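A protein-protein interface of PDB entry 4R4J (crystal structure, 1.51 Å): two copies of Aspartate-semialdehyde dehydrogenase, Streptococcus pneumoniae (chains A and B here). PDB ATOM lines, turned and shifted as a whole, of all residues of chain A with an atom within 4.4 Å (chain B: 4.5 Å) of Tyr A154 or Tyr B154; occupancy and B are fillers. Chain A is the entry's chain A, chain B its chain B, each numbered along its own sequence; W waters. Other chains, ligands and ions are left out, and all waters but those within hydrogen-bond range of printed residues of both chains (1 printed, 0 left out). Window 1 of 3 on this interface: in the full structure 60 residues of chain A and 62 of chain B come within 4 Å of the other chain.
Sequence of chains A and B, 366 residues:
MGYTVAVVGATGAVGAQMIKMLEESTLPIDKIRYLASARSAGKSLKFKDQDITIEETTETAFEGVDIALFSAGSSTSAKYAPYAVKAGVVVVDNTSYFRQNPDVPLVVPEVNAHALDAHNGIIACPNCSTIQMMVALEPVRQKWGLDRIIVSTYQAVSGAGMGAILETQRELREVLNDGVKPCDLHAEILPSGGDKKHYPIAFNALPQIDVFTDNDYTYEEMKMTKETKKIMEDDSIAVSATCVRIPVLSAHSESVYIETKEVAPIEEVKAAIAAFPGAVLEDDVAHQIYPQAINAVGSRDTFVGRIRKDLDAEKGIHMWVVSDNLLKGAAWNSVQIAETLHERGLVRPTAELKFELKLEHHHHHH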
ATOM      1  N   SER A 152     -10.638 -22.880   8.159  1.00  0.00           N
ATOM      2  CA  SER A 152     -10.510 -22.062   9.360  1.00  0.00           C
ATOM      3  C   SER A 152     -11.932 -21.753   9.839  1.00  0.00           C
ATOM      4  O   SER A 152     -12.760 -21.241   9.079  1.00  0.00           O
ATOM      5  CB  SER A 152      -9.753 -20.780   9.063  1.00  0.00           C
ATOM      6  OG  SER A 152      -8.417 -21.038   8.661  1.00  0.00           O
ATOM      7  N   THR A 153     -12.230 -22.104  11.087  1.00  0.00           N
ATOM      8  CA  THR A 153     -13.583 -21.974  11.602  1.00  0.00           C
ATOM      9  C   THR A 153     -13.795 -20.761  12.503  1.00  0.00           C
ATOM     10  O   THR A 153     -12.853 -20.179  13.051  1.00  0.00           O
ATOM     11  CB  THR A 153     -14.015 -23.221  12.372  1.00  0.00           C
ATOM     12  OG1 THR A 153     -13.395 -23.228  13.662  1.00  0.00           O
ATOM     13  CG2 THR A 153     -13.678 -24.485  11.607  1.00  0.00           C
ATOM     14  N   TYR A 154     -15.070 -20.400  12.618  1.00  0.00           N
ATOM     15  CA  TYR A 154     -15.537 -19.257  13.379  1.00  0.00           C
ATOM     16  C   TYR A 154     -16.708 -19.779  14.203  1.00  0.00           C
ATOM     17  O   TYR A 154     -17.876 -19.688  13.798  1.00  0.00           O
ATOM     18  CB  TYR A 154     -15.994 -18.124  12.443  1.00  0.00           C
ATOM     19  CG  TYR A 154     -14.931 -17.575  11.508  1.00  0.00           C
ATOM     20  CD1 TYR A 154     -14.388 -18.358  10.489  1.00  0.00           C
ATOM     21  CD2 TYR A 154     -14.515 -16.250  11.601  1.00  0.00           C
ATOM     22  CE1 TYR A 154     -13.419 -17.862   9.639  1.00  0.00           C
ATOM     23  CE2 TYR A 154     -13.560 -15.736  10.739  1.00  0.00           C
ATOM     24  CZ  TYR A 154     -13.028 -16.541   9.746  1.00  0.00           C
ATOM     25  OH  TYR A 154     -12.071 -16.044   8.890  1.00  0.00           O
ATOM     26  N   GLN A 155     -16.385 -20.374  15.345  1.00  0.00           N
ATOM     27  CA  GLN A 155     -17.340 -21.205  16.055  1.00  0.00           C
ATOM     28  C   GLN A 155     -18.036 -20.487  17.203  1.00  0.00           C
ATOM     29  O   GLN A 155     -17.407 -19.760  17.959  1.00  0.00           O
ATOM     30  CB  GLN A 155     -16.646 -22.492  16.537  1.00  0.00           C
ATOM     31  CG  GLN A 155     -16.344 -23.421  15.362  1.00  0.00           C
ATOM     32  CD  GLN A 155     -15.688 -24.758  15.708  1.00  0.00           C
ATOM     33  OE1 GLN A 155     -14.632 -25.090  15.175  1.00  0.00           O
ATOM     34  NE2 GLN A 155     -16.322 -25.535  16.565  1.00  0.00           N
ATOM     35  N   ALA A 156     -19.355 -20.685  17.273  1.00  0.00           N
ATOM     36  CA  ALA A 156     -20.220 -20.156  18.306  1.00  0.00           C
ATOM     37  C   ALA A 156     -20.021 -20.849  19.644  1.00  0.00           C
ATOM     38  O   ALA A 156     -19.711 -22.030  19.707  1.00  0.00           O
ATOM     39  CB  ALA A 156     -21.671 -20.285  17.863  1.00  0.00           C
ATOM     40  N   VAL A 244     -11.474 -22.003  15.760  1.00  0.00           N
ATOM     41  CA  VAL A 244     -11.422 -20.785  16.562  1.00  0.00           C
ATOM     42  C   VAL A 244     -12.806 -20.460  17.128  1.00  0.00           C
ATOM     43  O   VAL A 244     -13.812 -20.495  16.405  1.00  0.00           O
ATOM     44  CB  VAL A 244     -10.911 -19.587  15.719  1.00  0.00           C
ATOM     45  CG1 VAL A 244     -10.723 -18.339  16.568  1.00  0.00           C
ATOM     46  CG2 VAL A 244      -9.614 -19.926  15.002  1.00  0.00           C
ATOM     47  N   ILE A 246     -15.357 -17.675  18.536  1.00  0.00           N
ATOM     48  CA  ILE A 246     -15.601 -16.240  18.445  1.00  0.00           C
ATOM     49  C   ILE A 246     -16.850 -15.841  19.239  1.00  0.00           C
ATOM     50  O   ILE A 246     -17.595 -16.731  19.686  1.00  0.00           O
ATOM     51  CB  ILE A 246     -15.675 -15.753  16.983  1.00  0.00           C
ATOM     52  CG1 ILE A 246     -16.881 -16.334  16.224  1.00  0.00           C
ATOM     53  CG2 ILE A 246     -14.371 -16.091  16.266  1.00  0.00           C
ATOM     54  CD1 ILE A 246     -17.216 -15.555  14.977  1.00  0.00           C
ATOM     55  N   ALA A 251     -24.566 -20.701  15.714  1.00  0.00           N
ATOM     56  CA  ALA A 251     -24.206 -20.854  14.301  1.00  0.00           C
ATOM     57  C   ALA A 251     -22.718 -20.733  14.078  1.00  0.00           C
ATOM     58  O   ALA A 251     -22.108 -19.701  14.409  1.00  0.00           O
ATOM     59  CB  ALA A 251     -24.974 -19.921  13.368  1.00  0.00           C
ATOM     60  N   HIS A 252     -22.154 -21.795  13.499  1.00  0.00           N
ATOM     61  CA  HIS A 252     -20.739 -21.837  13.136  1.00  0.00           C
ATOM     62  C   HIS A 252     -20.572 -21.367  11.707  1.00  0.00           C
ATOM     63  O   HIS A 252     -21.383 -21.706  10.834  1.00  0.00           O
ATOM     64  CB  HIS A 252     -20.170 -23.254  13.193  1.00  0.00           C
ATOM     65  CG  HIS A 252     -20.072 -23.848  14.566  1.00  0.00           C
ATOM     66  ND1 HIS A 252     -20.192 -23.109  15.721  1.00  0.00           N
ATOM     67  CD2 HIS A 252     -19.803 -25.114  14.961  1.00  0.00           C
ATOM     68  CE1 HIS A 252     -20.031 -23.900  16.768  1.00  0.00           C
ATOM     69  NE2 HIS A 252     -19.791 -25.121  16.333  1.00  0.00           N
ATOM     70  N   SER A 253     -19.503 -20.624  11.468  1.00  0.00           N
ATOM     71  CA  SER A 253     -19.112 -20.221  10.124  1.00  0.00           C
ATOM     72  C   SER A 253     -17.727 -20.782   9.812  1.00  0.00           C
ATOM     73  O   SER A 253     -16.890 -20.949  10.707  1.00  0.00           O
ATOM     74  CB  SER A 253     -19.101 -18.691   9.983  1.00  0.00           C
ATOM     75  OG  SER A 253     -20.249 -18.077  10.551  1.00  0.00           O
ATOM     76  N   SER A 255     -14.472 -20.671   6.794  1.00  0.00           N
ATOM     77  CA  SER A 255     -13.758 -20.313   5.573  1.00  0.00           C
ATOM     78  C   SER A 255     -13.091 -21.581   5.054  1.00  0.00           C
ATOM     79  O   SER A 255     -12.177 -22.127   5.691  1.00  0.00           O
ATOM     80  CB  SER A 255     -12.709 -19.253   5.858  1.00  0.00           C
ATOM     81  OG  SER A 255     -11.995 -18.938   4.674  1.00  0.00           O
ATOM     82  N   TRP A 320     -17.619 -19.892   1.880  1.00  0.00           N
ATOM     83  CA  TRP A 320     -18.044 -19.537   3.230  1.00  0.00           C
ATOM     84  C   TRP A 320     -19.283 -20.373   3.552  1.00  0.00           C
ATOM     85  O   TRP A 320     -20.270 -20.326   2.820  1.00  0.00           O
ATOM     86  CB  TRP A 320     -18.385 -18.063   3.273  1.00  0.00           C
ATOM     87  CG  TRP A 320     -18.769 -17.474   4.605  1.00  0.00           C
ATOM     88  CD1 TRP A 320     -19.981 -16.962   4.944  1.00  0.00           C
ATOM     89  CD2 TRP A 320     -17.916 -17.253   5.740  1.00  0.00           C
ATOM     90  NE1 TRP A 320     -19.948 -16.449   6.219  1.00  0.00           N
ATOM     91  CE2 TRP A 320     -18.696 -16.627   6.733  1.00  0.00           C
ATOM     92  CE3 TRP A 320     -16.582 -17.543   6.018  1.00  0.00           C
ATOM     93  CZ2 TRP A 320     -18.174 -16.262   7.974  1.00  0.00           C
ATOM     94  CZ3 TRP A 320     -16.068 -17.201   7.259  1.00  0.00           C
ATOM     95  CH2 TRP A 320     -16.864 -16.586   8.222  1.00  0.00           C
ATOM     96  N   SER B 152      -7.266 -16.489   6.259  1.00  0.00           N
ATOM     97  CA  SER B 152      -8.622 -16.164   6.652  1.00  0.00           C
ATOM     98  C   SER B 152      -8.519 -15.270   7.869  1.00  0.00           C
ATOM     99  O   SER B 152      -7.847 -15.625   8.848  1.00  0.00           O
ATOM    100  CB  SER B 152      -9.414 -17.419   6.980  1.00  0.00           C
ATOM    101  OG  SER B 152      -9.594 -18.235   5.840  1.00  0.00           O
ATOM    102  N   THR B 153      -9.118 -14.088   7.776  1.00  0.00           N
ATOM    103  CA  THR B 153      -8.997 -13.091   8.844  1.00  0.00           C
ATOM    104  C   THR B 153     -10.212 -13.033   9.774  1.00  0.00           C
ATOM    105  O   THR B 153     -11.327 -13.453   9.429  1.00  0.00           O
ATOM    106  CB  THR B 153      -8.741 -11.679   8.299  1.00  0.00           C
ATOM    107  OG1 THR B 153      -9.960 -11.166   7.773  1.00  0.00           O
ATOM    108  CG2 THR B 153      -7.663 -11.680   7.213  1.00  0.00           C
ATOM    109  N   TYR B 154      -9.963 -12.468  10.951  1.00  0.00           N
ATOM    110  CA  TYR B 154     -10.933 -12.329  12.022  1.00  0.00           C
ATOM    111  C   TYR B 154     -10.769 -10.879  12.494  1.00  0.00           C
ATOM    112  O   TYR B 154     -10.037 -10.600  13.461  1.00  0.00           O
ATOM    113  CB  TYR B 154     -10.619 -13.315  13.165  1.00  0.00           C
ATOM    114  CG  TYR B 154     -10.657 -14.801  12.810  1.00  0.00           C
ATOM    115  CD1 TYR B 154      -9.736 -15.369  11.934  1.00  0.00           C
ATOM    116  CD2 TYR B 154     -11.589 -15.646  13.395  1.00  0.00           C
ATOM    117  CE1 TYR B 154      -9.775 -16.720  11.624  1.00  0.00           C
ATOM    118  CE2 TYR B 154     -11.629 -16.997  13.094  1.00  0.00           C
ATOM    119  CZ  TYR B 154     -10.722 -17.535  12.207  1.00  0.00           C
ATOM    120  OH  TYR B 154     -10.760 -18.878  11.916  1.00  0.00           O
ATOM    121  N   GLN B 155     -11.408  -9.958  11.789  1.00  0.00           N
ATOM    122  CA  GLN B 155     -11.078  -8.543  11.915  1.00  0.00           C
ATOM    123  C   GLN B 155     -11.986  -7.784  12.856  1.00  0.00           C
ATOM    124  O   GLN B 155     -13.197  -7.957  12.853  1.00  0.00           O
ATOM    125  CB  GLN B 155     -11.019  -7.892  10.527  1.00  0.00           C
ATOM    126  CG  GLN B 155      -9.773  -8.331   9.769  1.00  0.00           C
ATOM    127  CD  GLN B 155      -9.655  -7.800   8.356  1.00  0.00           C
ATOM    128  OE1 GLN B 155      -9.568  -8.575   7.401  1.00  0.00           O
ATOM    129  NE2 GLN B 155      -9.617  -6.482   8.215  1.00  0.00           N
ATOM    130  N   ALA B 156     -11.358  -6.957  13.684  1.00  0.00           N
ATOM    131  CA  ALA B 156     -12.027  -6.064  14.619  1.00  0.00           C
ATOM    132  C   ALA B 156     -12.747  -4.910  13.940  1.00  0.00           C
ATOM    133  O   ALA B 156     -12.318  -4.430  12.902  1.00  0.00           O
ATOM    134  CB  ALA B 156     -11.001  -5.520  15.597  1.00  0.00           C
ATOM    135  N   VAL B 244     -12.974 -11.379   7.110  1.00  0.00           N
ATOM    136  CA  VAL B 244     -14.209 -11.508   7.861  1.00  0.00           C
ATOM    137  C   VAL B 244     -14.187 -10.584   9.073  1.00  0.00           C
ATOM    138  O   VAL B 244     -13.213 -10.554   9.838  1.00  0.00           O
ATOM    139  CB  VAL B 244     -14.429 -12.971   8.328  1.00  0.00           C
ATOM    140  CG1 VAL B 244     -15.772 -13.118   9.011  1.00  0.00           C
ATOM    141  CG2 VAL B 244     -14.317 -13.944   7.155  1.00  0.00           C
ATOM    142  N   ILE B 246     -15.612  -9.760  12.739  1.00  0.00           N
ATOM    143  CA  ILE B 246     -16.215 -10.439  13.874  1.00  0.00           C
ATOM    144  C   ILE B 246     -16.463  -9.434  15.001  1.00  0.00           C
ATOM    145  O   ILE B 246     -15.989  -8.304  14.932  1.00  0.00           O
ATOM    146  CB  ILE B 246     -15.353 -11.629  14.356  1.00  0.00           C
ATOM    147  CG1 ILE B 246     -13.983 -11.174  14.876  1.00  0.00           C
ATOM    148  CG2 ILE B 246     -15.200 -12.668  13.249  1.00  0.00           C
ATOM    149  CD1 ILE B 246     -13.263 -12.213  15.703  1.00  0.00           C
ATOM    150  N   ALA B 251      -8.017  -5.246  17.588  1.00  0.00           N
ATOM    151  CA  ALA B 251      -7.049  -6.320  17.306  1.00  0.00           C
ATOM    152  C   ALA B 251      -7.584  -7.317  16.294  1.00  0.00           C
ATOM    153  O   ALA B 251      -8.647  -7.902  16.492  1.00  0.00           O
ATOM    154  CB  ALA B 251      -6.537  -7.022  18.563  1.00  0.00           C
ATOM    155  N   HIS B 252      -6.830  -7.472  15.203  1.00  0.00           N
ATOM    156  CA  HIS B 252      -7.130  -8.443  14.155  1.00  0.00           C
ATOM    157  C   HIS B 252      -6.408  -9.748  14.424  1.00  0.00           C
ATOM    158  O   HIS B 252      -5.233  -9.754  14.852  1.00  0.00           O
ATOM    159  CB  HIS B 252      -6.666  -7.965  12.770  1.00  0.00           C
ATOM    160  CG  HIS B 252      -7.391  -6.774  12.225  1.00  0.00           C
ATOM    161  ND1 HIS B 252      -8.587  -6.319  12.728  1.00  0.00           N
ATOM    162  CD2 HIS B 252      -7.078  -5.943  11.202  1.00  0.00           C
ATOM    163  CE1 HIS B 252      -8.983  -5.259  12.046  1.00  0.00           C
ATOM    164  NE2 HIS B 252      -8.088  -5.018  11.107  1.00  0.00           N
ATOM    165  N   SER B 253      -7.081 -10.854  14.120  1.00  0.00           N
ATOM    166  CA  SER B 253      -6.476 -12.178  14.191  1.00  0.00           C
ATOM    167  C   SER B 253      -6.525 -12.783  12.810  1.00  0.00           C
ATOM    168  O   SER B 253      -7.438 -12.470  12.033  1.00  0.00           O
ATOM    169  CB  SER B 253      -7.225 -13.066  15.191  1.00  0.00           C
ATOM    170  OG  SER B 253      -7.427 -12.381  16.418  1.00  0.00           O
ATOM    171  N   GLU B 254      -5.553 -13.628  12.494  1.00  0.00           N
ATOM    172  CA  GLU B 254      -5.476 -14.241  11.173  1.00  0.00           C
ATOM    173  C   GLU B 254      -5.044 -15.685  11.285  1.00  0.00           C
ATOM    174  O   GLU B 254      -4.046 -15.992  11.940  1.00  0.00           O
ATOM    175  CB  GLU B 254      -4.484 -13.477  10.291  1.00  0.00           C
ATOM    176  CG  GLU B 254      -4.869 -12.034  10.050  1.00  0.00           C
ATOM    177  CD  GLU B 254      -3.775 -11.213   9.403  1.00  0.00           C
ATOM    178  OE1 GLU B 254      -2.592 -11.587   9.510  1.00  0.00           O
ATOM    179  OE2 GLU B 254      -4.116 -10.173   8.806  1.00  0.00           O
ATOM    180  N   SER B 255      -5.798 -16.564  10.619  1.00  0.00           N
ATOM    181  CA  SER B 255      -5.386 -17.940  10.389  1.00  0.00           C
ATOM    182  C   SER B 255      -4.616 -17.960   9.066  1.00  0.00           C
ATOM    183  O   SER B 255      -5.186 -17.712   8.007  1.00  0.00           O
ATOM    184  CB  SER B 255      -6.592 -18.887  10.363  1.00  0.00           C
ATOM    185  OG  SER B 255      -6.215 -20.220  10.066  1.00  0.00           O
ATOM    186  N   TRP B 320      -1.172 -18.653  13.669  1.00  0.00           N
ATOM    187  CA  TRP B 320      -2.177 -17.709  14.154  1.00  0.00           C
ATOM    188  C   TRP B 320      -1.464 -16.414  14.475  1.00  0.00           C
ATOM    189  O   TRP B 320      -0.523 -16.409  15.279  1.00  0.00           O
ATOM    190  CB  TRP B 320      -2.810 -18.261  15.416  1.00  0.00           C
ATOM    191  CG  TRP B 320      -3.939 -17.471  16.018  1.00  0.00           C
ATOM    192  CD1 TRP B 320      -3.947 -16.837  17.234  1.00  0.00           C
ATOM    193  CD2 TRP B 320      -5.249 -17.282  15.464  1.00  0.00           C
ATOM    194  NE1 TRP B 320      -5.173 -16.276  17.469  1.00  0.00           N
ATOM    195  CE2 TRP B 320      -5.995 -16.535  16.401  1.00  0.00           C
ATOM    196  CE3 TRP B 320      -5.869 -17.691  14.274  1.00  0.00           C
ATOM    197  CZ2 TRP B 320      -7.321 -16.172  16.182  1.00  0.00           C
ATOM    198  CZ3 TRP B 320      -7.177 -17.305  14.044  1.00  0.00           C
ATOM    199  CH2 TRP B 320      -7.896 -16.566  14.998  1.00  0.00           C
HETATM  200  O   HOH W   1      -8.045 -20.452   6.136  1.00  0.00           O
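OG of Ser A152 sits at hydrogen-bond distance from OG of Ser B255.
The side-chain hydroxyl (OG) of Ser B152 sits at hydrogen-bond distance from the side-chain hydroxyl (OG) of Ser A255 (2.8 Å).
The backbone carbonyl oxygen (O) of Thr A153 is in hydrogen-bond range of the side-chain hydroxyl (OH) of Tyr B154 (2.7 Å).
The backbone carbonyl oxygen of Thr B153 is in hydrogen-bond range of the side-chain hydroxyl of Tyr A154, at 2.7 Å.
The backbone NH (N) of Val B244 sits at hydrogen-bond distance from the side-chain hydroxyl (OG1) of Thr B153 (3.1 Å).
O of Ser B253 lies within hydrogen-bond range of N of Tyr B154, at 2.7 Å.
The backbone carbonyl oxygen (O) of Ser B152 is in hydrogen-bond range of the backbone NH (N) of Ser B255.
The backbone carbonyl oxygen (O) of Ser A152 is in hydrogen-bond range of the backbone NH (N) of Ser A255 (2.9 Å).
O of Gln A155 lies within hydrogen-bond range of N of Ile A246 (3.0 Å).
The backbone carbonyl oxygen of Val A244 is in hydrogen-bond range of the backbone NH of Gln A155 (2.8 Å).
Among the printed residues, merely in contact across the chains: Tyr A154 with Tyr B154 (3.3 Å), Val A244 with Tyr B154 (3.5 Å), Tyr A154 with Val B244 (3.5 Å), Tyr A154 with Ser B152 (3.5 Å), Ser A152 with Tyr B154 (3.6 Å), Val A244 with Trp B320 (3.7 Å), Trp A320 with Val B244 (3.7 Å), Ile A246 with Ile B246 (3.9 Å) and Ser A152 with Ser B152 (3.97 Å).
Of chain A, only Ser A152 (3.6 Å), Thr A153 (2.7 Å), Tyr A154 (3.3 Å) and Val A244 (3.5 Å) come within 4 Å of Tyr B154.
Printed residues of chain B within 4 Å of Ile A246: Ile B246 (3.9 Å).
Of the printed residues of chain B, Thr A153 touches Tyr B154 (2.7 Å).
Of the 13 printed residues of chain B, 7 touch a printed residue of chain A.
Hydrophobic or aromatic side chains of chain B that line the printed part of chain A: Tyr B154, Val B244, Ile B246 and Trp B320.
Among the printed residues, 13 pairs touch across the chains.
Among the printed residues, no Asp or Glu carboxylate lies within 4 Å of a Lys or Arg side-chain nitrogen of the other chain.
Ser B152 touches its own counterpart, Ser A152.
Thr A153 touches Tyr B154, and with the chains exchanged Tyr A154 touches Thr B153.
Tyr B154 touches its own counterpart, Tyr A154.
Val A244 touches Trp B320, and with the chains exchanged Trp A320 touches Val B244.
Of the 13 pairs that touch across the chains among the printed residues, 13 have their exchanged pair printed and touching as well.
Water W1 lies within hydrogen-bond range of OG of Ser A152 (2.6 Å) and OG of Ser B152 (2.7 Å).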
